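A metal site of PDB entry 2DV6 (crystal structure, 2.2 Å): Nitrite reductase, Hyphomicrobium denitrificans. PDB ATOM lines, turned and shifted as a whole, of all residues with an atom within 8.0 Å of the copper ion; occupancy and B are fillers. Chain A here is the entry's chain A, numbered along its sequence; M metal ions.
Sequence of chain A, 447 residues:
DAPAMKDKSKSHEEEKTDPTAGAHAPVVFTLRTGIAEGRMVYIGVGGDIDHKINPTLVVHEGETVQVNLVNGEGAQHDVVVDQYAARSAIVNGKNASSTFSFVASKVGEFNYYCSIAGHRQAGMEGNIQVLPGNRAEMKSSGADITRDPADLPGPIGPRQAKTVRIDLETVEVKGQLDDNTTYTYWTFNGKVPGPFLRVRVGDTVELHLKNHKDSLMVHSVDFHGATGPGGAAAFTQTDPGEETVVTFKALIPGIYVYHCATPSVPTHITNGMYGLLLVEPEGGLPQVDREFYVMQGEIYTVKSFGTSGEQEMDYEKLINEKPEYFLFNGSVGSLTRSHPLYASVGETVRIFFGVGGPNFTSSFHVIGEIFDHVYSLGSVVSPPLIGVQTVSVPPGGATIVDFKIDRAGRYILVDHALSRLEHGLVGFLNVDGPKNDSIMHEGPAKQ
Within 4 Å of the copper ion: His 219, Cys 260, His 268 and Met 273.
The nearest printed residue that does not touch the copper ion is Val 218 (4.1 Å).
ND1 of His 268 is bound to the copper ion.
The copper ion is bound by the side-chain sulfur (SG) of Cys 260, 2.1 Å away.
The copper ion is bound by ND1 of His 219 (2.1 Å).
SD of Met 273 binds the copper ion (2.5 Å).
The copper ion has four donor atoms within binding distance.
O of His 219 sits at hydrogen-bond distance from N of Thr 238, 2.8 Å away.
The side-chain sulfur of Cys 260 sits close to the backbone NH of Ser 220 (3.4 Å).
The backbone NH of Met 273 sits close to the backbone carbonyl oxygen of Trp 186 (3.3 Å).
The side-chain sulfur (SG) of Cys 260 lies close to the backbone NH (N) of Thr 262.
NE2 of His 268 lies close to O of Thr 262, at 3.5 Å.
The side-chain carboxylate (OE1) of Glu 172 is in hydrogen-bond range of a ring nitrogen (NE2) of His 219, 2.7 Å away.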
ATOM      1  N   THR A 170     -14.266  10.433 -18.321  1.00  0.00           N
ATOM      2  CA  THR A 170     -14.617   9.083 -17.884  1.00  0.00           C
ATOM      3  C   THR A 170     -14.015   8.070 -18.837  1.00  0.00           C
ATOM      4  O   THR A 170     -14.265   8.111 -20.044  1.00  0.00           O
ATOM      5  CB  THR A 170     -16.141   8.886 -17.701  1.00  0.00           C
ATOM      6  OG1 THR A 170     -16.823   9.203 -18.937  1.00  0.00           O
ATOM      7  CG2 THR A 170     -16.634   9.829 -16.615  1.00  0.00           C
ATOM      8  N   VAL A 171     -13.135   7.223 -18.308  1.00  0.00           N
ATOM      9  CA  VAL A 171     -12.450   6.226 -19.121  1.00  0.00           C
ATOM     10  C   VAL A 171     -12.551   4.822 -18.544  1.00  0.00           C
ATOM     11  O   VAL A 171     -12.305   4.626 -17.362  1.00  0.00           O
ATOM     12  CB  VAL A 171     -10.940   6.665 -19.534  1.00  0.00           C
ATOM     13  CG1 VAL A 171     -10.499   7.898 -18.888  1.00  0.00           C
ATOM     14  CG2 VAL A 171      -9.925   5.594 -19.289  1.00  0.00           C
ATOM     15  N   GLU A 172     -12.900   3.870 -19.411  1.00  0.00           N
ATOM     16  CA  GLU A 172     -12.898   2.434 -19.129  1.00  0.00           C
ATOM     17  C   GLU A 172     -11.562   1.842 -19.602  1.00  0.00           C
ATOM     18  O   GLU A 172     -11.169   1.981 -20.753  1.00  0.00           O
ATOM     19  CB  GLU A 172     -14.102   1.748 -19.805  1.00  0.00           C
ATOM     20  CG  GLU A 172     -15.443   2.495 -19.500  1.00  0.00           C
ATOM     21  CD  GLU A 172     -16.599   2.066 -20.407  1.00  0.00           C
ATOM     22  OE1 GLU A 172     -17.679   2.647 -20.274  1.00  0.00           O
ATOM     23  OE2 GLU A 172     -16.440   1.147 -21.233  1.00  0.00           O
ATOM     24  N   TRP A 186     -13.519   1.416 -14.409  1.00  0.00           N
ATOM     25  CA  TRP A 186     -14.152   2.582 -14.984  1.00  0.00           C
ATOM     26  C   TRP A 186     -13.760   3.714 -14.072  1.00  0.00           C
ATOM     27  O   TRP A 186     -13.918   3.624 -12.850  1.00  0.00           O
ATOM     28  CB  TRP A 186     -15.695   2.441 -15.025  1.00  0.00           C
ATOM     29  CG  TRP A 186     -16.207   1.246 -15.834  1.00  0.00           C
ATOM     30  CD1 TRP A 186     -15.504   0.458 -16.698  1.00  0.00           C
ATOM     31  CD2 TRP A 186     -17.556   0.787 -15.874  1.00  0.00           C
ATOM     32  NE1 TRP A 186     -16.330  -0.493 -17.246  1.00  0.00           N
ATOM     33  CE2 TRP A 186     -17.604  -0.298 -16.771  1.00  0.00           C
ATOM     34  CE3 TRP A 186     -18.729   1.165 -15.219  1.00  0.00           C
ATOM     35  CZ2 TRP A 186     -18.799  -1.026 -17.029  1.00  0.00           C
ATOM     36  CZ3 TRP A 186     -19.916   0.447 -15.488  1.00  0.00           C
ATOM     37  CH2 TRP A 186     -19.929  -0.626 -16.363  1.00  0.00           C
ATOM     38  N   THR A 187     -13.260   4.792 -14.652  1.00  0.00           N
ATOM     39  CA  THR A 187     -12.579   5.772 -13.825  1.00  0.00           C
ATOM     40  C   THR A 187     -12.922   7.185 -14.228  1.00  0.00           C
ATOM     41  O   THR A 187     -13.318   7.444 -15.366  1.00  0.00           O
ATOM     42  CB  THR A 187     -11.037   5.650 -14.000  1.00  0.00           C
ATOM     43  OG1 THR A 187     -10.715   6.013 -15.344  1.00  0.00           O
ATOM     44  CG2 THR A 187     -10.521   4.227 -13.702  1.00  0.00           C
ATOM     45  N   PHE A 188     -12.725   8.105 -13.291  1.00  0.00           N
ATOM     46  CA  PHE A 188     -12.530   9.514 -13.609  1.00  0.00           C
ATOM     47  C   PHE A 188     -11.040   9.772 -13.834  1.00  0.00           C
ATOM     48  O   PHE A 188     -10.236   9.580 -12.929  1.00  0.00           O
ATOM     49  CB  PHE A 188     -13.051  10.397 -12.473  1.00  0.00           C
ATOM     50  CG  PHE A 188     -14.545  10.313 -12.277  1.00  0.00           C
ATOM     51  CD1 PHE A 188     -15.424  10.901 -13.223  1.00  0.00           C
ATOM     52  CD2 PHE A 188     -15.072   9.657 -11.157  1.00  0.00           C
ATOM     53  CE1 PHE A 188     -16.814  10.845 -13.037  1.00  0.00           C
ATOM     54  CE2 PHE A 188     -16.455   9.584 -10.963  1.00  0.00           C
ATOM     55  CZ  PHE A 188     -17.346  10.170 -11.903  1.00  0.00           C
ATOM     56  N   LEU A 209     -17.552  17.550 -18.269  1.00  0.00           N
ATOM     57  CA  LEU A 209     -17.419  16.095 -18.229  1.00  0.00           C
ATOM     58  C   LEU A 209     -17.371  15.526 -19.634  1.00  0.00           C
ATOM     59  O   LEU A 209     -18.373  15.616 -20.368  1.00  0.00           O
ATOM     60  CB  LEU A 209     -18.561  15.441 -17.439  1.00  0.00           C
ATOM     61  CG  LEU A 209     -18.353  13.930 -17.074  1.00  0.00           C
ATOM     62  CD1 LEU A 209     -19.409  13.481 -16.094  1.00  0.00           C
ATOM     63  CD2 LEU A 209     -18.472  13.055 -18.271  1.00  0.00           C
ATOM     64  N   ASN A 211     -16.928  12.021 -21.914  1.00  0.00           N
ATOM     65  CA  ASN A 211     -16.938  10.568 -21.866  1.00  0.00           C
ATOM     66  C   ASN A 211     -16.123  10.092 -23.052  1.00  0.00           C
ATOM     67  O   ASN A 211     -16.460  10.367 -24.182  1.00  0.00           O
ATOM     68  CB  ASN A 211     -18.373  10.027 -21.852  1.00  0.00           C
ATOM     69  CG  ASN A 211     -18.449   8.540 -21.609  1.00  0.00           C
ATOM     70  OD1 ASN A 211     -17.437   7.869 -21.333  1.00  0.00           O
ATOM     71  ND2 ASN A 211     -19.655   7.989 -21.699  1.00  0.00           N
ATOM     72  N   MET A 217     -20.142   2.547 -22.039  1.00  0.00           N
ATOM     73  CA  MET A 217     -21.249   2.911 -21.164  1.00  0.00           C
ATOM     74  C   MET A 217     -21.414   4.413 -21.174  1.00  0.00           C
ATOM     75  O   MET A 217     -20.433   5.144 -21.360  1.00  0.00           O
ATOM     76  CB  MET A 217     -20.993   2.457 -19.705  1.00  0.00           C
ATOM     77  CG  MET A 217     -20.640   0.994 -19.551  1.00  0.00           C
ATOM     78  SD  MET A 217     -21.940  -0.034 -20.270  1.00  0.00           S
ATOM     79  CE  MET A 217     -21.258  -1.698 -19.982  1.00  0.00           C
ATOM     80  N   VAL A 218     -22.621   4.890 -20.918  1.00  0.00           N
ATOM     81  CA  VAL A 218     -22.708   6.262 -20.458  1.00  0.00           C
ATOM     82  C   VAL A 218     -22.178   6.438 -19.031  1.00  0.00           C
ATOM     83  O   VAL A 218     -22.216   5.479 -18.230  1.00  0.00           O
ATOM     84  CB  VAL A 218     -24.090   6.967 -20.727  1.00  0.00           C
ATOM     85  CG1 VAL A 218     -24.986   6.189 -21.687  1.00  0.00           C
ATOM     86  CG2 VAL A 218     -24.775   7.568 -19.490  1.00  0.00           C
ATOM     87  N   HIS A 219     -21.613   7.614 -18.753  1.00  0.00           N
ATOM     88  CA  HIS A 219     -21.104   7.939 -17.421  1.00  0.00           C
ATOM     89  C   HIS A 219     -21.571   9.362 -17.041  1.00  0.00           C
ATOM     90  O   HIS A 219     -22.021  10.110 -17.903  1.00  0.00           O
ATOM     91  CB  HIS A 219     -19.575   7.797 -17.318  1.00  0.00           C
ATOM     92  CG  HIS A 219     -19.054   6.422 -17.645  1.00  0.00           C
ATOM     93  ND1 HIS A 219     -19.109   5.366 -16.756  1.00  0.00           N
ATOM     94  CD2 HIS A 219     -18.467   5.943 -18.755  1.00  0.00           C
ATOM     95  CE1 HIS A 219     -18.576   4.294 -17.309  1.00  0.00           C
ATOM     96  NE2 HIS A 219     -18.189   4.608 -18.534  1.00  0.00           N
ATOM     97  N   SER A 220     -21.530   9.669 -15.750  1.00  0.00           N
ATOM     98  CA  SER A 220     -22.012  10.941 -15.222  1.00  0.00           C
ATOM     99  C   SER A 220     -21.265  11.176 -13.946  1.00  0.00           C
ATOM    100  O   SER A 220     -20.280  10.464 -13.658  1.00  0.00           O
ATOM    101  CB  SER A 220     -23.515  10.866 -14.919  1.00  0.00           C
ATOM    102  OG  SER A 220     -23.772   9.758 -14.087  1.00  0.00           O
ATOM    103  N   VAL A 221     -21.737  12.133 -13.158  1.00  0.00           N
ATOM    104  CA  VAL A 221     -21.172  12.434 -11.853  1.00  0.00           C
ATOM    105  C   VAL A 221     -22.252  13.030 -10.932  1.00  0.00           C
ATOM    106  O   VAL A 221     -23.059  13.824 -11.361  1.00  0.00           O
ATOM    107  CB  VAL A 221     -19.900  13.361 -11.954  1.00  0.00           C
ATOM    108  CG1 VAL A 221     -20.258  14.750 -12.658  1.00  0.00           C
ATOM    109  CG2 VAL A 221     -19.297  13.590 -10.557  1.00  0.00           C
ATOM    110  N   GLN A 237     -25.443  12.997 -17.608  1.00  0.00           N
ATOM    111  CA  GLN A 237     -25.485  11.692 -18.295  1.00  0.00           C
ATOM    112  C   GLN A 237     -24.823  11.885 -19.654  1.00  0.00           C
ATOM    113  O   GLN A 237     -25.394  12.551 -20.508  1.00  0.00           O
ATOM    114  CB  GLN A 237     -26.923  11.176 -18.456  1.00  0.00           C
ATOM    115  CG  GLN A 237     -27.675  10.978 -17.100  1.00  0.00           C
ATOM    116  CD  GLN A 237     -26.924  10.003 -16.163  1.00  0.00           C
ATOM    117  OE1 GLN A 237     -26.678  10.297 -14.963  1.00  0.00           O
ATOM    118  NE2 GLN A 237     -26.502   8.874 -16.711  1.00  0.00           N
ATOM    119  N   THR A 238     -23.616  11.333 -19.844  1.00  0.00           N
ATOM    120  CA  THR A 238     -22.770  11.672 -21.001  1.00  0.00           C
ATOM    121  C   THR A 238     -22.495  10.445 -21.861  1.00  0.00           C
ATOM    122  O   THR A 238     -21.955   9.448 -21.372  1.00  0.00           O
ATOM    123  CB  THR A 238     -21.439  12.317 -20.507  1.00  0.00           C
ATOM    124  OG1 THR A 238     -21.750  13.321 -19.533  1.00  0.00           O
ATOM    125  CG2 THR A 238     -20.679  12.969 -21.620  1.00  0.00           C
ATOM    126  N   HIS A 259     -19.280  10.547  -7.217  1.00  0.00           N
ATOM    127  CA  HIS A 259     -19.196   9.270  -7.906  1.00  0.00           C
ATOM    128  C   HIS A 259     -20.046   9.305  -9.165  1.00  0.00           C
ATOM    129  O   HIS A 259     -20.926  10.163  -9.307  1.00  0.00           O
ATOM    130  CB  HIS A 259     -19.680   8.141  -6.960  1.00  0.00           C
ATOM    131  CG  HIS A 259     -21.015   8.407  -6.350  1.00  0.00           C
ATOM    132  ND1 HIS A 259     -22.201   8.187  -7.027  1.00  0.00           N
ATOM    133  CD2 HIS A 259     -21.361   8.884  -5.130  1.00  0.00           C
ATOM    134  CE1 HIS A 259     -23.220   8.498  -6.246  1.00  0.00           C
ATOM    135  NE2 HIS A 259     -22.737   8.933  -5.089  1.00  0.00           N
ATOM    136  N   CYS A 260     -19.813   8.376 -10.081  1.00  0.00           N
ATOM    137  CA  CYS A 260     -20.704   8.259 -11.224  1.00  0.00           C
ATOM    138  C   CYS A 260     -22.100   7.933 -10.719  1.00  0.00           C
ATOM    139  O   CYS A 260     -22.276   7.243  -9.715  1.00  0.00           O
ATOM    140  CB  CYS A 260     -20.217   7.176 -12.172  1.00  0.00           C
ATOM    141  SG  CYS A 260     -21.207   6.959 -13.673  1.00  0.00           S
ATOM    142  N   ALA A 261     -23.094   8.466 -11.418  1.00  0.00           N
ATOM    143  CA  ALA A 261     -24.480   8.232 -11.057  1.00  0.00           C
ATOM    144  C   ALA A 261     -25.296   7.692 -12.240  1.00  0.00           C
ATOM    145  O   ALA A 261     -26.481   8.018 -12.390  1.00  0.00           O
ATOM    146  CB  ALA A 261     -25.123   9.518 -10.475  1.00  0.00           C
ATOM    147  N   THR A 262     -24.682   6.830 -13.054  1.00  0.00           N
ATOM    148  CA  THR A 262     -25.410   6.163 -14.132  1.00  0.00           C
ATOM    149  C   THR A 262     -25.849   4.739 -13.698  1.00  0.00           C
ATOM    150  O   THR A 262     -25.045   3.985 -13.204  1.00  0.00           O
ATOM    151  CB  THR A 262     -24.527   6.094 -15.394  1.00  0.00           C
ATOM    152  OG1 THR A 262     -24.186   7.449 -15.759  1.00  0.00           O
ATOM    153  CG2 THR A 262     -25.248   5.341 -16.591  1.00  0.00           C
ATOM    154  N   PRO A 263     -27.139   4.397 -13.848  1.00  0.00           N
ATOM    155  CA  PRO A 263     -27.565   3.023 -13.523  1.00  0.00           C
ATOM    156  C   PRO A 263     -26.733   1.998 -14.302  1.00  0.00           C
ATOM    157  O   PRO A 263     -26.455   2.242 -15.451  1.00  0.00           O
ATOM    158  CB  PRO A 263     -29.018   3.000 -13.984  1.00  0.00           C
ATOM    159  CG  PRO A 263     -29.446   4.432 -13.825  1.00  0.00           C
ATOM    160  CD  PRO A 263     -28.274   5.239 -14.278  1.00  0.00           C
ATOM    161  N   SER A 264     -26.263   0.904 -13.702  1.00  0.00           N
ATOM    162  CA  SER A 264     -26.332   0.554 -12.282  1.00  0.00           C
ATOM    163  C   SER A 264     -25.323   1.369 -11.476  1.00  0.00           C
ATOM    164  O   SER A 264     -24.113   1.254 -11.688  1.00  0.00           O
ATOM    165  CB  SER A 264     -26.011  -0.940 -12.166  1.00  0.00           C
ATOM    166  OG  SER A 264     -25.677  -1.348 -10.833  1.00  0.00           O
ATOM    167  N   VAL A 265     -25.796   2.205 -10.565  1.00  0.00           N
ATOM    168  CA  VAL A 265     -24.846   3.027  -9.819  1.00  0.00           C
ATOM    169  C   VAL A 265     -23.822   2.197  -9.024  1.00  0.00           C
ATOM    170  O   VAL A 265     -22.638   2.477  -9.146  1.00  0.00           O
ATOM    171  CB  VAL A 265     -25.519   4.107  -8.912  1.00  0.00           C
ATOM    172  CG1 VAL A 265     -24.439   4.927  -8.213  1.00  0.00           C
ATOM    173  CG2 VAL A 265     -26.408   5.061  -9.766  1.00  0.00           C
ATOM    174  N   THR A 267     -22.654  -0.640  -9.625  1.00  0.00           N
ATOM    175  CA  THR A 267     -21.712  -1.134 -10.631  1.00  0.00           C
ATOM    176  C   THR A 267     -20.664  -0.098 -11.088  1.00  0.00           C
ATOM    177  O   THR A 267     -19.493  -0.417 -11.169  1.00  0.00           O
ATOM    178  CB  THR A 267     -22.457  -1.625 -11.878  1.00  0.00           C
ATOM    179  OG1 THR A 267     -23.429  -2.649 -11.517  1.00  0.00           O
ATOM    180  CG2 THR A 267     -21.437  -2.161 -12.919  1.00  0.00           C
ATOM    181  N   HIS A 268     -21.088   1.127 -11.415  1.00  0.00           N
ATOM    182  CA  HIS A 268     -20.131   2.169 -11.799  1.00  0.00           C
ATOM    183  C   HIS A 268     -19.168   2.490 -10.639  1.00  0.00           C
ATOM    184  O   HIS A 268     -17.982   2.733 -10.872  1.00  0.00           O
ATOM    185  CB  HIS A 268     -20.859   3.458 -12.301  1.00  0.00           C
ATOM    186  CG  HIS A 268     -21.523   3.273 -13.646  1.00  0.00           C
ATOM    187  ND1 HIS A 268     -21.033   3.840 -14.800  1.00  0.00           N
ATOM    188  CD2 HIS A 268     -22.576   2.508 -14.015  1.00  0.00           C
ATOM    189  CE1 HIS A 268     -21.775   3.459 -15.831  1.00  0.00           C
ATOM    190  NE2 HIS A 268     -22.706   2.643 -15.389  1.00  0.00           N
ATOM    191  N   ILE A 269     -19.680   2.491  -9.408  1.00  0.00           N
ATOM    192  CA  ILE A 269     -18.865   2.743  -8.210  1.00  0.00           C
ATOM    193  C   ILE A 269     -17.882   1.617  -7.951  1.00  0.00           C
ATOM    194  O   ILE A 269     -16.661   1.861  -7.825  1.00  0.00           O
ATOM    195  CB  ILE A 269     -19.726   2.999  -6.971  1.00  0.00           C
ATOM    196  CG1 ILE A 269     -20.393   4.358  -7.089  1.00  0.00           C
ATOM    197  CG2 ILE A 269     -18.877   2.941  -5.660  1.00  0.00           C
ATOM    198  CD1 ILE A 269     -21.485   4.565  -6.029  1.00  0.00           C
ATOM    199  N   ASN A 271     -16.558  -0.396  -9.992  1.00  0.00           N
ATOM    200  CA  ASN A 271     -15.537  -0.407 -11.047  1.00  0.00           C
ATOM    201  C   ASN A 271     -14.498   0.726 -10.943  1.00  0.00           C
ATOM    202  O   ASN A 271     -13.527   0.750 -11.693  1.00  0.00           O
ATOM    203  CB  ASN A 271     -16.170  -0.366 -12.442  1.00  0.00           C
ATOM    204  CG  ASN A 271     -16.904  -1.641 -12.806  1.00  0.00           C
ATOM    205  OD1 ASN A 271     -17.813  -1.630 -13.647  1.00  0.00           O
ATOM    206  ND2 ASN A 271     -16.508  -2.751 -12.199  1.00  0.00           N
ATOM    207  N   GLY A 272     -14.729   1.688 -10.058  1.00  0.00           N
ATOM    208  CA  GLY A 272     -13.755   2.736  -9.745  1.00  0.00           C
ATOM    209  C   GLY A 272     -14.202   4.194  -9.746  1.00  0.00           C
ATOM    210  O   GLY A 272     -13.390   5.114  -9.485  1.00  0.00           O
ATOM    211  N   MET A 273     -15.474   4.456 -10.058  1.00  0.00           N
ATOM    212  CA  MET A 273     -15.903   5.862 -10.293  1.00  0.00           C
ATOM    213  C   MET A 273     -16.328   6.595  -9.033  1.00  0.00           C
ATOM    214  O   MET A 273     -17.524   6.832  -8.771  1.00  0.00           O
ATOM    215  CB  MET A 273     -16.969   5.962 -11.391  1.00  0.00           C
ATOM    216  CG  MET A 273     -16.601   5.216 -12.626  1.00  0.00           C
ATOM    217  SD  MET A 273     -17.532   5.533 -14.121  1.00  0.00           S
ATOM    218  CE  MET A 273     -16.911   7.221 -14.455  1.00  0.00           C
HETATM  219 CU    CU M   1     -19.980   5.654 -14.815  1.00  0.00          CU
